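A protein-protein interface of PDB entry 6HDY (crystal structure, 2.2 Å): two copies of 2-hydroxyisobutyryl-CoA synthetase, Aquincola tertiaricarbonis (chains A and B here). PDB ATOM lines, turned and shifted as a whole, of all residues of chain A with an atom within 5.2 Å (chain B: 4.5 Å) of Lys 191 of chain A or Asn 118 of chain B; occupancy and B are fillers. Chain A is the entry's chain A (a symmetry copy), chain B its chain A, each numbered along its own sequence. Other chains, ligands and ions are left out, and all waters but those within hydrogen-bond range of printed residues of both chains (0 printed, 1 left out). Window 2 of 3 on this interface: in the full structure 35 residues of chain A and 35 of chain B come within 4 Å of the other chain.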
ATOM      1  N   GLY A 163     -18.194  -6.357 -19.226  1.00  0.00           N
ATOM      2  CA  GLY A 163     -18.670  -6.748 -20.544  1.00  0.00           C
ATOM      3  C   GLY A 163     -18.918  -8.225 -20.698  1.00  0.00           C
ATOM      4  O   GLY A 163     -19.545  -8.631 -21.673  1.00  0.00           O
ATOM      5  N   ASP A 164     -18.409  -9.048 -19.770  1.00  0.00           N
ATOM      6  CA  ASP A 164     -18.682 -10.489 -19.798  1.00  0.00           C
ATOM      7  C   ASP A 164     -20.153 -10.743 -19.479  1.00  0.00           C
ATOM      8  O   ASP A 164     -20.715 -10.120 -18.577  1.00  0.00           O
ATOM      9  CB  ASP A 164     -17.861 -11.218 -18.744  1.00  0.00           C
ATOM     10  CG  ASP A 164     -16.419 -11.509 -19.103  1.00  0.00           C
ATOM     11  OD1 ASP A 164     -16.062 -11.396 -20.315  1.00  0.00           O
ATOM     12  OD2 ASP A 164     -15.666 -11.930 -18.199  1.00  0.00           O
ATOM     13  N   LEU A 165     -20.767 -11.671 -20.209  1.00  0.00           N
ATOM     14  CA  LEU A 165     -22.140 -12.072 -19.980  1.00  0.00           C
ATOM     15  C   LEU A 165     -22.135 -13.067 -18.796  1.00  0.00           C
ATOM     16  O   LEU A 165     -21.489 -14.126 -18.867  1.00  0.00           O
ATOM     17  CB  LEU A 165     -22.760 -12.687 -21.240  1.00  0.00           C
ATOM     18  CG  LEU A 165     -24.246 -13.080 -21.083  1.00  0.00           C
ATOM     19  CD1 LEU A 165     -25.113 -11.895 -21.192  1.00  0.00           C
ATOM     20  CD2 LEU A 165     -24.665 -14.050 -22.150  1.00  0.00           C
ATOM     21  N   VAL A 166     -22.822 -12.693 -17.691  1.00  0.00           N
ATOM     22  CA  VAL A 166     -22.870 -13.510 -16.480  1.00  0.00           C
ATOM     23  C   VAL A 166     -24.265 -14.069 -16.312  1.00  0.00           C
ATOM     24  O   VAL A 166     -25.201 -13.304 -16.074  1.00  0.00           O
ATOM     25  CB  VAL A 166     -22.412 -12.731 -15.216  1.00  0.00           C
ATOM     26  CG1 VAL A 166     -22.477 -13.621 -13.965  1.00  0.00           C
ATOM     27  CG2 VAL A 166     -21.012 -12.159 -15.400  1.00  0.00           C
ATOM     28  N   ARG A 189     -19.751  -4.286 -13.956  1.00  0.00           N
ATOM     29  CA  ARG A 189     -20.081  -3.771 -15.281  1.00  0.00           C
ATOM     30  C   ARG A 189     -20.102  -4.940 -16.283  1.00  0.00           C
ATOM     31  O   ARG A 189     -19.779  -4.789 -17.460  1.00  0.00           O
ATOM     32  CB  ARG A 189     -19.193  -2.573 -15.735  1.00  0.00           C
ATOM     33  CG  ARG A 189     -18.972  -1.482 -14.678  1.00  0.00           C
ATOM     34  CD  ARG A 189     -20.177  -0.590 -14.456  1.00  0.00           C
ATOM     35  NE  ARG A 189     -20.093   0.165 -13.200  1.00  0.00           N
ATOM     36  CZ  ARG A 189     -21.008   0.124 -12.229  1.00  0.00           C
ATOM     37  NH1 ARG A 189     -20.855   0.858 -11.135  1.00  0.00           N
ATOM     38  NH2 ARG A 189     -22.100  -0.628 -12.362  1.00  0.00           N
ATOM     39  N   ALA A 190     -20.496  -6.124 -15.798  1.00  0.00           N
ATOM     40  CA  ALA A 190     -20.650  -7.292 -16.656  1.00  0.00           C
ATOM     41  C   ALA A 190     -22.051  -7.145 -17.274  1.00  0.00           C
ATOM     42  O   ALA A 190     -22.803  -6.277 -16.849  1.00  0.00           O
ATOM     43  CB  ALA A 190     -20.569  -8.571 -15.806  1.00  0.00           C
ATOM     44  N   LYS A 191     -22.395  -7.944 -18.283  1.00  0.00           N
ATOM     45  CA  LYS A 191     -23.761  -7.955 -18.815  1.00  0.00           C
ATOM     46  C   LYS A 191     -24.510  -8.949 -17.889  1.00  0.00           C
ATOM     47  O   LYS A 191     -24.361 -10.169 -18.041  1.00  0.00           O
ATOM     48  CB  LYS A 191     -23.791  -8.450 -20.271  1.00  0.00           C
ATOM     49  CG  LYS A 191     -23.185  -7.506 -21.277  1.00  0.00           C
ATOM     50  CD  LYS A 191     -23.028  -8.229 -22.602  1.00  0.00           C
ATOM     51  CE  LYS A 191     -22.391  -7.372 -23.662  1.00  0.00           C
ATOM     52  NZ  LYS A 191     -21.055  -6.850 -23.256  1.00  0.00           N
ATOM     53  N   ALA A 192     -25.210  -8.434 -16.858  1.00  0.00           N
ATOM     54  CA  ALA A 192     -25.897  -9.329 -15.898  1.00  0.00           C
ATOM     55  C   ALA A 192     -27.075 -10.011 -16.578  1.00  0.00           C
ATOM     56  O   ALA A 192     -27.909  -9.336 -17.170  1.00  0.00           O
ATOM     57  CB  ALA A 192     -26.356  -8.556 -14.662  1.00  0.00           C
ATOM     58  N   PHE A 193     -27.085 -11.356 -16.573  1.00  0.00           N
ATOM     59  CA  PHE A 193     -28.147 -12.156 -17.183  1.00  0.00           C
ATOM     60  C   PHE A 193     -28.901 -12.943 -16.063  1.00  0.00           C
ATOM     61  O   PHE A 193     -28.622 -14.136 -15.827  1.00  0.00           O
ATOM     62  CB  PHE A 193     -27.558 -13.071 -18.293  1.00  0.00           C
ATOM     63  CG  PHE A 193     -28.520 -14.039 -18.938  1.00  0.00           C
ATOM     64  CD1 PHE A 193     -29.859 -13.698 -19.127  1.00  0.00           C
ATOM     65  CD2 PHE A 193     -28.077 -15.271 -19.415  1.00  0.00           C
ATOM     66  CE1 PHE A 193     -30.753 -14.597 -19.723  1.00  0.00           C
ATOM     67  CE2 PHE A 193     -28.962 -16.160 -20.044  1.00  0.00           C
ATOM     68  CZ  PHE A 193     -30.298 -15.823 -20.191  1.00  0.00           C
ATOM     69  N   VAL B 116     -26.804   1.358 -28.429  1.00  0.00           N
ATOM     70  CA  VAL B 116     -25.697   1.553 -27.500  1.00  0.00           C
ATOM     71  C   VAL B 116     -24.568   0.579 -27.821  1.00  0.00           C
ATOM     72  O   VAL B 116     -24.847  -0.493 -28.377  1.00  0.00           O
ATOM     73  CB  VAL B 116     -26.158   1.430 -26.011  1.00  0.00           C
ATOM     74  CG1 VAL B 116     -27.118   2.546 -25.620  1.00  0.00           C
ATOM     75  CG2 VAL B 116     -26.717   0.050 -25.681  1.00  0.00           C
ATOM     76  N   PRO B 117     -23.297   0.881 -27.450  1.00  0.00           N
ATOM     77  CA  PRO B 117     -22.246  -0.122 -27.651  1.00  0.00           C
ATOM     78  C   PRO B 117     -22.486  -1.292 -26.708  1.00  0.00           C
ATOM     79  O   PRO B 117     -23.150  -1.136 -25.682  1.00  0.00           O
ATOM     80  CB  PRO B 117     -20.952   0.615 -27.274  1.00  0.00           C
ATOM     81  CG  PRO B 117     -21.326   2.066 -27.151  1.00  0.00           C
ATOM     82  CD  PRO B 117     -22.768   2.081 -26.764  1.00  0.00           C
ATOM     83  N   ASN B 118     -21.928  -2.456 -27.052  1.00  0.00           N
ATOM     84  CA  ASN B 118     -21.987  -3.691 -26.269  1.00  0.00           C
ATOM     85  C   ASN B 118     -21.601  -3.464 -24.802  1.00  0.00           C
ATOM     86  O   ASN B 118     -22.252  -3.991 -23.913  1.00  0.00           O
ATOM     87  CB  ASN B 118     -21.062  -4.738 -26.891  1.00  0.00           C
ATOM     88  CG  ASN B 118     -21.672  -6.114 -26.963  1.00  0.00           C
ATOM     89  OD1 ASN B 118     -22.875  -6.282 -27.237  1.00  0.00           O
ATOM     90  ND2 ASN B 118     -20.840  -7.131 -26.733  1.00  0.00           N
ATOM     91  N   SER B 119     -20.569  -2.649 -24.567  1.00  0.00           N
ATOM     92  CA  SER B 119     -20.035  -2.280 -23.260  1.00  0.00           C
ATOM     93  C   SER B 119     -21.024  -1.522 -22.376  1.00  0.00           C
ATOM     94  O   SER B 119     -20.797  -1.404 -21.176  1.00  0.00           O
ATOM     95  CB  SER B 119     -18.743  -1.478 -23.428  1.00  0.00           C
ATOM     96  OG  SER B 119     -18.984  -0.195 -23.982  1.00  0.00           O
ATOM     97  N   GLU B 120     -22.102  -0.990 -22.953  1.00  0.00           N
ATOM     98  CA  GLU B 120     -23.087  -0.245 -22.180  1.00  0.00           C
ATOM     99  C   GLU B 120     -24.175  -1.183 -21.577  1.00  0.00           C
ATOM    100  O   GLU B 120     -24.814  -0.799 -20.584  1.00  0.00           O
ATOM    101  CB  GLU B 120     -23.654   0.916 -23.034  1.00  0.00           C
ATOM    102  CG  GLU B 120     -24.983   1.546 -22.610  1.00  0.00           C
ATOM    103  CD  GLU B 120     -25.040   2.530 -21.453  1.00  0.00           C
ATOM    104  OE1 GLU B 120     -23.979   2.856 -20.868  1.00  0.00           O
ATOM    105  OE2 GLU B 120     -26.163   2.995 -21.148  1.00  0.00           O
ATOM    106  N   ILE B 121     -24.366  -2.401 -22.155  1.00  0.00           N
ATOM    107  CA  ILE B 121     -25.418  -3.343 -21.712  1.00  0.00           C
ATOM    108  C   ILE B 121     -25.215  -3.760 -20.249  1.00  0.00           C
ATOM    109  O   ILE B 121     -24.129  -4.218 -19.848  1.00  0.00           O
ATOM    110  CB  ILE B 121     -25.618  -4.547 -22.672  1.00  0.00           C
ATOM    111  CG1 ILE B 121     -26.072  -4.040 -24.062  1.00  0.00           C
ATOM    112  CG2 ILE B 121     -26.658  -5.555 -22.113  1.00  0.00           C
ATOM    113  CD1 ILE B 121     -25.405  -4.747 -25.163  1.00  0.00           C
ATOM    114  N   PHE B 122     -26.257  -3.504 -19.467  1.00  0.00           N
ATOM    115  CA  PHE B 122     -26.338  -3.723 -18.031  1.00  0.00           C
ATOM    116  C   PHE B 122     -27.075  -5.013 -17.658  1.00  0.00           C
ATOM    117  O   PHE B 122     -26.609  -5.743 -16.795  1.00  0.00           O
ATOM    118  CB  PHE B 122     -27.037  -2.506 -17.384  1.00  0.00           C
ATOM    119  CG  PHE B 122     -27.217  -2.506 -15.885  1.00  0.00           C
ATOM    120  CD1 PHE B 122     -26.118  -2.416 -15.033  1.00  0.00           C
ATOM    121  CD2 PHE B 122     -28.479  -2.584 -15.323  1.00  0.00           C
ATOM    122  CE1 PHE B 122     -26.286  -2.391 -13.644  1.00  0.00           C
ATOM    123  CE2 PHE B 122     -28.648  -2.564 -13.930  1.00  0.00           C
ATOM    124  CZ  PHE B 122     -27.550  -2.419 -13.105  1.00  0.00           C
ATOM    125  N   VAL B 124     -29.636  -8.413 -19.183  1.00  0.00           N
ATOM    126  CA  VAL B 124     -30.125  -9.266 -20.261  1.00  0.00           C
ATOM    127  C   VAL B 124     -31.405  -9.933 -19.784  1.00  0.00           C
ATOM    128  O   VAL B 124     -31.411 -10.592 -18.752  1.00  0.00           O
ATOM    129  CB  VAL B 124     -29.090 -10.280 -20.812  1.00  0.00           C
ATOM    130  CG1 VAL B 124     -29.696 -11.146 -21.917  1.00  0.00           C
ATOM    131  CG2 VAL B 124     -27.833  -9.566 -21.315  1.00  0.00           C
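The side-chain amino group (NZ) of Lys 191 of chain A lies within hydrogen-bond range of the backbone carbonyl oxygen (O) of Asn 118 of chain B, at 3.2 Å.
N of Ala 192 of chain A sits at hydrogen-bond distance from O of Phe 122 of chain B (3.0 Å).
The backbone carbonyl oxygen (O) of Ala 192 of chain A is in hydrogen-bond range of the backbone NH (N) of Val 124 of chain B.
O of Gly 163 of chain A lies within hydrogen-bond range of NZ of Lys 191 of chain A (2.8 Å).
The backbone carbonyl oxygen (O) of Asp 164 of chain A lies within hydrogen-bond range of the backbone NH (N) of Lys 191 of chain A.
The backbone carbonyl oxygen (O) of Lys 191 of chain A is in hydrogen-bond range of the backbone NH (N) of Val 166 of chain A.
The backbone carbonyl oxygen of Val 166 of chain A is in hydrogen-bond range of the backbone NH of Phe 193 of chain A, at 2.8 Å.
Among the printed residues, pairs that only touch across the chains: Leu 165 of chain A with Val 124 of chain B (3.6 Å), Ala 190 of chain A with Ile 121 of chain B (3.9 Å), Ala 190 of chain A with Phe 122 of chain B (3.8 Å), Lys 191 of chain A with Ile 121 of chain B (3.7 Å), Lys 191 of chain A with Phe 122 of chain B (3.99 Å) and Phe 193 of chain A with Val 124 of chain B (3.5 Å).
Of the printed residues of chain B, Lys 191 of chain A touches Asn 118, Ile 121 and Phe 122.
Asn 118 of chain B touches one residue of chain A.
Printed residues of chain B within 4 Å of Ala 192 of chain A: Phe 122 (3.0 Å) and Val 124 (2.8 Å).
Of the printed residues of chain B, Ala 190 of chain A touches Ile 121 (3.9 Å) and Phe 122 (3.8 Å).
Of the printed residues of chain A, Val 124 of chain B touches Leu 165, Ala 192 and Phe 193.
Arg 189 of chain A touches none of the printed residues of chain B.
Ser 119 of chain B touches none of the printed residues of chain A.
The nearest printed residue of chain A that does not touch Val 124 of chain B is Lys 191 of chain A (4.3 Å).
Hydrophobic or aromatic side chains of chain A within 4 Å of the printed part of chain B: Leu 165, Ala 192 and Phe 193.
Hydrophobic or aromatic side chains of chain B within 4 Å of the printed part of chain A: Val 124.
Among the printed residues, 9 pairs touch across the chains.
No position is printed for both chains.
Of the 9 pairs that touch across the chains among the printed residues, none has its exchanged pair printed and touching as well.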
